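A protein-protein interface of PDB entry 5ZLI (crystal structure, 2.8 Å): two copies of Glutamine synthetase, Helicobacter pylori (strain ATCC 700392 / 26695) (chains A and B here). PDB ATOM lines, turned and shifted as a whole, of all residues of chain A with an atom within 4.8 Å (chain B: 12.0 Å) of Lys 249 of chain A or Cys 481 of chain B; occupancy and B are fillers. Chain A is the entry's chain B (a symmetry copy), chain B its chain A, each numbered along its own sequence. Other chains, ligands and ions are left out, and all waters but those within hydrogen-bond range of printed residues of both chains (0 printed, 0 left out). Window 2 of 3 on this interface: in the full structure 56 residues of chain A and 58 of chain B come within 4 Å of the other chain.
O of Ser 480 of chain B lies within hydrogen-bond range of NZ of Lys 253 of chain A (3.3 Å). N of Met 266 of chain A is in hydrogen-bond range of SG of Cys 481 of chain B (3.7 Å). NZ of Lys 253 of chain A sits at hydrogen-bond distance from O of Cys 481 of chain B (2.9 Å).
OG1 of Thr 478 of chain B sits close to O of Glu 474 of chain B (3.3 Å). The backbone carbonyl oxygen of Ser 373 of chain A is in hydrogen-bond range of the side-chain amino group of Lys 249 of chain A (2.8 Å). The backbone carbonyl oxygen (O) of Thr 478 of chain B sits close to the side-chain sulfur (SG) of Cys 481 of chain B, 3.1 Å away.
Among the printed residues, pairs that only touch across the chains: Lys 249 of chain A with Cys 481 of chain B (3.6 Å), Phe 265 of chain A with Cys 481 of chain B (3.8 Å), Met 266 of chain A with Phe 475 of chain B (3.5 Å), Met 266 of chain A with Thr 478 of chain B (3.9 Å), Met 266 of chain A with Tyr 479 of chain B (3.98 Å), Ser 374 of chain A with Thr 478 of chain B (3.9 Å) and Ser 374 of chain A with Cys 481 of chain B (3.9 Å).
Lys 249 of chain A touches just one residue of chain B: Cys 481 (3.6 Å). Cys 481 of chain B touches five residues of chain A. No residue of chain B comes within 4 Å of Asn 140 of chain A. No residue of chain B comes within 4 Å of Val 245 of chain A. Lys 253 of chain A touches just these residues of chain B: Ser 480 (3.3 Å) and Cys 481 (2.9 Å). Phe 265 of chain A touches just one residue of chain B: Cys 481. Met 266 of chain A touches four residues of chain B. No residue of chain B comes within 4 Å of Ser 373 of chain A. No residue of chain B comes within 4 Å of Ser 375 of chain A. Of the printed residues of chain A, Ser 480 of chain B touches Lys 253 (3.3 Å). Printed residues of chain A within 4 Å of Tyr 479 of chain B: Met 266. Printed residues of chain A within 4 Å of Thr 478 of chain B: Met 266 and Ser 374. Printed residues of chain A within 4 Å of Phe 475 of chain B: Met 266. Ile 476 of chain B touches none of the printed residues of chain A. The nearest residue of chain A that does not touch Cys 481 of chain B is Ser 373 of chain A (4.1 Å). The nearest printed residue of chain A that does not touch Ser 480 of chain B is Phe 265 of chain A (6.1 Å).
Printed residues of chain B that touch a printed residue of chain A: Phe 475, Thr 478, Tyr 479, Ser 480 and Cys 481. Of the 16 printed residues of chain A, 5 touch a printed residue of chain B. Among the printed residues, 10 pairs touch across the chains. Among the printed residues, no Asp or Glu carboxylate lies within 4 Å of a Lys or Arg side-chain nitrogen of the other chain.
No position is printed for both chains.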
ATOM      1  N   ASN A 140     -16.147  -6.720  -9.230  1.00  0.00           N
ATOM      2  CA  ASN A 140     -17.349  -6.900  -8.406  1.00  0.00           C
ATOM      3  C   ASN A 140     -17.482  -8.369  -8.033  1.00  0.00           C
ATOM      4  O   ASN A 140     -18.072  -9.167  -8.765  1.00  0.00           O
ATOM      5  CB  ASN A 140     -18.616  -6.430  -9.106  1.00  0.00           C
ATOM      6  CG  ASN A 140     -18.632  -4.952  -9.359  1.00  0.00           C
ATOM      7  OD1 ASN A 140     -19.099  -4.177  -8.522  1.00  0.00           O
ATOM      8  ND2 ASN A 140     -18.151  -4.548 -10.537  1.00  0.00           N
ATOM      9  N   VAL A 245     -20.383  -2.009 -15.303  1.00  0.00           N
ATOM     10  CA  VAL A 245     -20.802  -2.581 -14.035  1.00  0.00           C
ATOM     11  C   VAL A 245     -22.295  -2.883 -14.065  1.00  0.00           C
ATOM     12  O   VAL A 245     -22.714  -3.985 -13.698  1.00  0.00           O
ATOM     13  CB  VAL A 245     -20.410  -1.647 -12.882  1.00  0.00           C
ATOM     14  CG1 VAL A 245     -21.132  -2.024 -11.577  1.00  0.00           C
ATOM     15  CG2 VAL A 245     -18.872  -1.639 -12.722  1.00  0.00           C
ATOM     16  N   GLN A 246     -23.121  -1.932 -14.537  1.00  0.00           N
ATOM     17  CA  GLN A 246     -24.556  -2.220 -14.686  1.00  0.00           C
ATOM     18  C   GLN A 246     -24.804  -3.456 -15.556  1.00  0.00           C
ATOM     19  O   GLN A 246     -25.598  -4.326 -15.194  1.00  0.00           O
ATOM     20  CB  GLN A 246     -25.333  -1.020 -15.262  1.00  0.00           C
ATOM     21  CG  GLN A 246     -25.443   0.219 -14.376  1.00  0.00           C
ATOM     22  CD  GLN A 246     -25.992  -0.051 -12.962  1.00  0.00           C
ATOM     23  OE1 GLN A 246     -25.269  -0.554 -12.104  1.00  0.00           O
ATOM     24  NE2 GLN A 246     -27.279   0.232 -12.740  1.00  0.00           N
ATOM     25  N   LYS A 247     -24.139  -3.545 -16.716  1.00  0.00           N
ATOM     26  CA  LYS A 247     -24.290  -4.718 -17.586  1.00  0.00           C
ATOM     27  C   LYS A 247     -23.870  -6.002 -16.864  1.00  0.00           C
ATOM     28  O   LYS A 247     -24.615  -6.986 -16.852  1.00  0.00           O
ATOM     29  CB  LYS A 247     -23.472  -4.558 -18.866  1.00  0.00           C
ATOM     30  CG  LYS A 247     -23.901  -3.492 -19.857  1.00  0.00           C
ATOM     31  CD  LYS A 247     -23.200  -3.809 -21.212  1.00  0.00           C
ATOM     32  CE  LYS A 247     -23.215  -2.644 -22.193  1.00  0.00           C
ATOM     33  NZ  LYS A 247     -22.602  -2.974 -23.488  1.00  0.00           N
ATOM     34  N   LEU A 248     -22.640  -6.025 -16.329  1.00  0.00           N
ATOM     35  CA  LEU A 248     -22.127  -7.160 -15.562  1.00  0.00           C
ATOM     36  C   LEU A 248     -23.090  -7.637 -14.468  1.00  0.00           C
ATOM     37  O   LEU A 248     -23.356  -8.844 -14.356  1.00  0.00           O
ATOM     38  CB  LEU A 248     -20.765  -6.785 -14.961  1.00  0.00           C
ATOM     39  CG  LEU A 248     -19.851  -7.619 -14.033  1.00  0.00           C
ATOM     40  CD1 LEU A 248     -20.278  -7.675 -12.568  1.00  0.00           C
ATOM     41  CD2 LEU A 248     -19.751  -9.007 -14.528  1.00  0.00           C
ATOM     42  N   LYS A 249     -23.594  -6.718 -13.623  1.00  0.00           N
ATOM     43  CA  LYS A 249     -24.549  -7.121 -12.579  1.00  0.00           C
ATOM     44  C   LYS A 249     -25.771  -7.821 -13.179  1.00  0.00           C
ATOM     45  O   LYS A 249     -26.158  -8.910 -12.748  1.00  0.00           O
ATOM     46  CB  LYS A 249     -24.973  -5.908 -11.733  1.00  0.00           C
ATOM     47  CG  LYS A 249     -23.930  -5.416 -10.682  1.00  0.00           C
ATOM     48  CD  LYS A 249     -24.444  -4.172  -9.946  1.00  0.00           C
ATOM     49  CE  LYS A 249     -23.363  -3.526  -9.039  1.00  0.00           C
ATOM     50  NZ  LYS A 249     -23.752  -2.188  -8.411  1.00  0.00           N
ATOM     51  N   TYR A 250     -26.341  -7.234 -14.219  1.00  0.00           N
ATOM     52  CA  TYR A 250     -27.456  -7.839 -14.937  1.00  0.00           C
ATOM     53  C   TYR A 250     -27.095  -9.213 -15.500  1.00  0.00           C
ATOM     54  O   TYR A 250     -27.910 -10.136 -15.466  1.00  0.00           O
ATOM     55  CB  TYR A 250     -27.858  -6.877 -16.056  1.00  0.00           C
ATOM     56  CG  TYR A 250     -28.888  -7.358 -17.027  1.00  0.00           C
ATOM     57  CD1 TYR A 250     -30.161  -7.717 -16.613  1.00  0.00           C
ATOM     58  CD2 TYR A 250     -28.598  -7.410 -18.399  1.00  0.00           C
ATOM     59  CE1 TYR A 250     -31.128  -8.143 -17.532  1.00  0.00           C
ATOM     60  CE2 TYR A 250     -29.565  -7.843 -19.332  1.00  0.00           C
ATOM     61  CZ  TYR A 250     -30.821  -8.203 -18.883  1.00  0.00           C
ATOM     62  OH  TYR A 250     -31.766  -8.621 -19.776  1.00  0.00           O
ATOM     63  N   VAL A 251     -25.871  -9.373 -16.015  1.00  0.00           N
ATOM     64  CA  VAL A 251     -25.538 -10.588 -16.748  1.00  0.00           C
ATOM     65  C   VAL A 251     -25.390 -11.761 -15.805  1.00  0.00           C
ATOM     66  O   VAL A 251     -25.745 -12.891 -16.142  1.00  0.00           O
ATOM     67  CB  VAL A 251     -24.282 -10.388 -17.613  1.00  0.00           C
ATOM     68  CG1 VAL A 251     -23.836 -11.699 -18.198  1.00  0.00           C
ATOM     69  CG2 VAL A 251     -24.575  -9.425 -18.742  1.00  0.00           C
ATOM     70  N   VAL A 252     -24.731 -11.553 -14.682  1.00  0.00           N
ATOM     71  CA  VAL A 252     -24.620 -12.651 -13.744  1.00  0.00           C
ATOM     72  C   VAL A 252     -25.976 -12.928 -13.090  1.00  0.00           C
ATOM     73  O   VAL A 252     -26.371 -14.090 -12.951  1.00  0.00           O
ATOM     74  CB  VAL A 252     -23.481 -12.398 -12.743  1.00  0.00           C
ATOM     75  CG1 VAL A 252     -22.353 -11.627 -13.412  1.00  0.00           C
ATOM     76  CG2 VAL A 252     -23.961 -11.659 -11.599  1.00  0.00           C
ATOM     77  N   LYS A 253     -26.743 -11.887 -12.750  1.00  0.00           N
ATOM     78  CA  LYS A 253     -28.031 -12.122 -12.092  1.00  0.00           C
ATOM     79  C   LYS A 253     -28.945 -12.964 -12.967  1.00  0.00           C
ATOM     80  O   LYS A 253     -29.641 -13.877 -12.491  1.00  0.00           O
ATOM     81  CB  LYS A 253     -28.738 -10.807 -11.754  1.00  0.00           C
ATOM     82  CG  LYS A 253     -28.615 -10.405 -10.265  1.00  0.00           C
ATOM     83  CD  LYS A 253     -29.154  -9.003 -10.012  1.00  0.00           C
ATOM     84  CE  LYS A 253     -28.300  -7.940 -10.602  1.00  0.00           C
ATOM     85  NZ  LYS A 253     -28.651  -6.642 -10.009  1.00  0.00           N
ATOM     86  N   PHE A 265     -24.845  -9.119  -5.457  1.00  0.00           N
ATOM     87  CA  PHE A 265     -23.581  -8.448  -5.216  1.00  0.00           C
ATOM     88  C   PHE A 265     -23.528  -7.752  -3.852  1.00  0.00           C
ATOM     89  O   PHE A 265     -22.594  -6.970  -3.618  1.00  0.00           O
ATOM     90  CB  PHE A 265     -23.286  -7.454  -6.311  1.00  0.00           C
ATOM     91  CG  PHE A 265     -23.042  -8.067  -7.660  1.00  0.00           C
ATOM     92  CD1 PHE A 265     -24.086  -8.565  -8.409  1.00  0.00           C
ATOM     93  CD2 PHE A 265     -21.790  -8.042  -8.229  1.00  0.00           C
ATOM     94  CE1 PHE A 265     -23.866  -9.054  -9.655  1.00  0.00           C
ATOM     95  CE2 PHE A 265     -21.576  -8.532  -9.476  1.00  0.00           C
ATOM     96  CZ  PHE A 265     -22.597  -9.034 -10.189  1.00  0.00           C
ATOM     97  N   MET A 266     -24.452  -8.091  -2.916  1.00  0.00           N
ATOM     98  CA  MET A 266     -24.518  -7.405  -1.620  1.00  0.00           C
ATOM     99  C   MET A 266     -23.257  -7.648  -0.784  1.00  0.00           C
ATOM    100  O   MET A 266     -22.713  -8.754  -0.776  1.00  0.00           O
ATOM    101  CB  MET A 266     -25.771  -7.836  -0.830  1.00  0.00           C
ATOM    102  CG  MET A 266     -25.759  -9.219  -0.174  1.00  0.00           C
ATOM    103  SD  MET A 266     -27.319  -9.683   0.649  1.00  0.00           S
ATOM    104  CE  MET A 266     -27.303  -8.572   2.014  1.00  0.00           C
ATOM    105  N   SER A 373     -20.426  -3.208  -4.124  1.00  0.00           N
ATOM    106  CA  SER A 373     -21.370  -3.080  -5.233  1.00  0.00           C
ATOM    107  C   SER A 373     -22.736  -2.572  -4.802  1.00  0.00           C
ATOM    108  O   SER A 373     -23.562  -2.254  -5.664  1.00  0.00           O
ATOM    109  CB  SER A 373     -21.520  -4.411  -5.966  1.00  0.00           C
ATOM    110  OG  SER A 373     -20.251  -4.930  -6.361  1.00  0.00           O
ATOM    111  N   SER A 374     -22.978  -2.419  -3.503  1.00  0.00           N
ATOM    112  CA  SER A 374     -24.175  -1.710  -3.066  1.00  0.00           C
ATOM    113  C   SER A 374     -24.105  -0.242  -3.447  1.00  0.00           C
ATOM    114  O   SER A 374     -25.067   0.503  -3.235  1.00  0.00           O
ATOM    115  CB  SER A 374     -24.378  -1.912  -1.549  1.00  0.00           C
ATOM    116  OG  SER A 374     -24.441  -0.703  -0.814  1.00  0.00           O
ATOM    117  N   SER A 375     -22.956   0.203  -3.917  1.00  0.00           N
ATOM    118  CA  SER A 375     -22.797   1.573  -4.354  1.00  0.00           C
ATOM    119  C   SER A 375     -23.377   1.772  -5.749  1.00  0.00           C
ATOM    120  O   SER A 375     -23.275   0.900  -6.616  1.00  0.00           O
ATOM    121  CB  SER A 375     -21.311   1.918  -4.333  1.00  0.00           C
ATOM    122  OG  SER A 375     -20.607   1.013  -5.172  1.00  0.00           O
ATOM    123  N   PRO A 377     -22.513   2.762  -9.045  1.00  0.00           N
ATOM    124  CA  PRO A 377     -21.210   2.934  -9.721  1.00  0.00           C
ATOM    125  C   PRO A 377     -20.977   4.332 -10.296  1.00  0.00           C
ATOM    126  O   PRO A 377     -19.841   4.828 -10.270  1.00  0.00           O
ATOM    127  CB  PRO A 377     -21.259   1.866 -10.827  1.00  0.00           C
ATOM    128  CG  PRO A 377     -22.714   1.559 -10.993  1.00  0.00           C
ATOM    129  CD  PRO A 377     -23.306   1.679  -9.632  1.00  0.00           C
ATOM    130  N   PRO B 472     -31.862  -9.277   8.225  1.00  0.00           N
ATOM    131  CA  PRO B 472     -32.748  -9.703   7.130  1.00  0.00           C
ATOM    132  C   PRO B 472     -33.318  -8.577   6.274  1.00  0.00           C
ATOM    133  O   PRO B 472     -33.713  -8.815   5.137  1.00  0.00           O
ATOM    134  CB  PRO B 472     -33.873 -10.450   7.866  1.00  0.00           C
ATOM    135  CG  PRO B 472     -33.733 -10.059   9.322  1.00  0.00           C
ATOM    136  CD  PRO B 472     -32.281  -9.823   9.527  1.00  0.00           C
ATOM    137  N   PHE B 473     -33.363  -7.350   6.767  1.00  0.00           N
ATOM    138  CA  PHE B 473     -33.930  -6.295   5.934  1.00  0.00           C
ATOM    139  C   PHE B 473     -32.965  -5.842   4.847  1.00  0.00           C
ATOM    140  O   PHE B 473     -33.382  -5.365   3.785  1.00  0.00           O
ATOM    141  CB  PHE B 473     -34.328  -5.118   6.804  1.00  0.00           C
ATOM    142  CG  PHE B 473     -35.136  -4.095   6.085  1.00  0.00           C
ATOM    143  CD1 PHE B 473     -36.427  -4.392   5.667  1.00  0.00           C
ATOM    144  CD2 PHE B 473     -34.651  -2.816   5.902  1.00  0.00           C
ATOM    145  CE1 PHE B 473     -37.201  -3.441   5.026  1.00  0.00           C
ATOM    146  CE2 PHE B 473     -35.406  -1.875   5.256  1.00  0.00           C
ATOM    147  CZ  PHE B 473     -36.690  -2.174   4.829  1.00  0.00           C
ATOM    148  N   GLU B 474     -31.677  -5.982   5.090  1.00  0.00           N
ATOM    149  CA  GLU B 474     -30.713  -5.660   4.056  1.00  0.00           C
ATOM    150  C   GLU B 474     -30.919  -6.549   2.838  1.00  0.00           C
ATOM    151  O   GLU B 474     -30.706  -6.114   1.701  1.00  0.00           O
ATOM    152  CB  GLU B 474     -29.326  -5.792   4.677  1.00  0.00           C
ATOM    153  CG  GLU B 474     -29.272  -4.958   5.952  1.00  0.00           C
ATOM    154  CD  GLU B 474     -28.019  -5.101   6.777  1.00  0.00           C
ATOM    155  OE1 GLU B 474     -27.590  -4.069   7.335  1.00  0.00           O
ATOM    156  OE2 GLU B 474     -27.459  -6.211   6.882  1.00  0.00           O
ATOM    157  N   PHE B 475     -31.449  -7.751   3.057  1.00  0.00           N
ATOM    158  CA  PHE B 475     -31.774  -8.645   1.960  1.00  0.00           C
ATOM    159  C   PHE B 475     -33.005  -8.188   1.192  1.00  0.00           C
ATOM    160  O   PHE B 475     -33.146  -8.495   0.012  1.00  0.00           O
ATOM    161  CB  PHE B 475     -31.990 -10.055   2.484  1.00  0.00           C
ATOM    162  CG  PHE B 475     -30.759 -10.675   3.029  1.00  0.00           C
ATOM    163  CD1 PHE B 475     -30.330 -10.377   4.307  1.00  0.00           C
ATOM    164  CD2 PHE B 475     -29.993 -11.508   2.245  1.00  0.00           C
ATOM    165  CE1 PHE B 475     -29.184 -10.927   4.816  1.00  0.00           C
ATOM    166  CE2 PHE B 475     -28.839 -12.067   2.751  1.00  0.00           C
ATOM    167  CZ  PHE B 475     -28.437 -11.780   4.038  1.00  0.00           C
ATOM    168  N   ILE B 476     -33.937  -7.507   1.829  1.00  0.00           N
ATOM    169  CA  ILE B 476     -35.017  -6.960   1.031  1.00  0.00           C
ATOM    170  C   ILE B 476     -34.511  -5.795   0.218  1.00  0.00           C
ATOM    171  O   ILE B 476     -34.895  -5.627  -0.946  1.00  0.00           O
ATOM    172  CB  ILE B 476     -36.197  -6.564   1.928  1.00  0.00           C
ATOM    173  CG1 ILE B 476     -36.780  -7.821   2.582  1.00  0.00           C
ATOM    174  CG2 ILE B 476     -37.248  -5.831   1.119  1.00  0.00           C
ATOM    175  CD1 ILE B 476     -37.584  -7.525   3.795  1.00  0.00           C
ATOM    176  N   THR B 477     -33.604  -5.007   0.792  1.00  0.00           N
ATOM    177  CA  THR B 477     -33.146  -3.776   0.158  1.00  0.00           C
ATOM    178  C   THR B 477     -32.093  -4.060  -0.884  1.00  0.00           C
ATOM    179  O   THR B 477     -32.236  -3.678  -2.045  1.00  0.00           O
ATOM    180  CB  THR B 477     -32.561  -2.827   1.220  1.00  0.00           C
ATOM    181  OG1 THR B 477     -33.589  -2.378   2.111  1.00  0.00           O
ATOM    182  CG2 THR B 477     -31.873  -1.614   0.564  1.00  0.00           C
ATOM    183  N   THR B 478     -31.058  -4.789  -0.481  1.00  0.00           N
ATOM    184  CA  THR B 478     -29.802  -4.790  -1.193  1.00  0.00           C
ATOM    185  C   THR B 478     -29.541  -6.056  -1.990  1.00  0.00           C
ATOM    186  O   THR B 478     -28.821  -5.989  -3.003  1.00  0.00           O
ATOM    187  CB  THR B 478     -28.640  -4.578  -0.203  1.00  0.00           C
ATOM    188  OG1 THR B 478     -28.945  -3.488   0.691  1.00  0.00           O
ATOM    189  CG2 THR B 478     -27.349  -4.321  -0.913  1.00  0.00           C
ATOM    190  N   TYR B 479     -30.195  -7.169  -1.648  1.00  0.00           N
ATOM    191  CA  TYR B 479     -29.913  -8.424  -2.338  1.00  0.00           C
ATOM    192  C   TYR B 479     -29.882  -8.223  -3.840  1.00  0.00           C
ATOM    193  O   TYR B 479     -29.030  -8.781  -4.529  1.00  0.00           O
ATOM    194  CB  TYR B 479     -30.954  -9.470  -1.986  1.00  0.00           C
ATOM    195  CG  TYR B 479     -30.617 -10.884  -2.440  1.00  0.00           C
ATOM    196  CD1 TYR B 479     -29.830 -11.734  -1.654  1.00  0.00           C
ATOM    197  CD2 TYR B 479     -31.102 -11.373  -3.632  1.00  0.00           C
ATOM    198  CE1 TYR B 479     -29.545 -13.030  -2.055  1.00  0.00           C
ATOM    199  CE2 TYR B 479     -30.821 -12.663  -4.042  1.00  0.00           C
ATOM    200  CZ  TYR B 479     -30.046 -13.490  -3.254  1.00  0.00           C
ATOM    201  OH  TYR B 479     -29.780 -14.768  -3.697  1.00  0.00           O
ATOM    202  N   SER B 480     -30.786  -7.404  -4.356  1.00  0.00           N
ATOM    203  CA  SER B 480     -30.881  -7.108  -5.776  1.00  0.00           C
ATOM    204  C   SER B 480     -29.975  -5.948  -6.210  1.00  0.00           C
ATOM    205  O   SER B 480     -30.108  -5.474  -7.338  1.00  0.00           O
ATOM    206  CB  SER B 480     -32.334  -6.807  -6.136  1.00  0.00           C
ATOM    207  OG  SER B 480     -33.120  -7.965  -5.933  1.00  0.00           O
ATOM    208  N   CYS B 481     -29.095  -5.456  -5.343  1.00  0.00           N
ATOM    209  CA  CYS B 481     -28.179  -4.377  -5.754  1.00  0.00           C
ATOM    210  C   CYS B 481     -27.153  -4.767  -6.855  1.00  0.00           C
ATOM    211  O   CYS B 481     -27.452  -4.878  -8.049  1.00  0.00           O
ATOM    212  CB  CYS B 481     -27.406  -3.847  -4.534  1.00  0.00           C
ATOM    213  SG  CYS B 481     -26.077  -4.977  -3.925  1.00  0.00           S
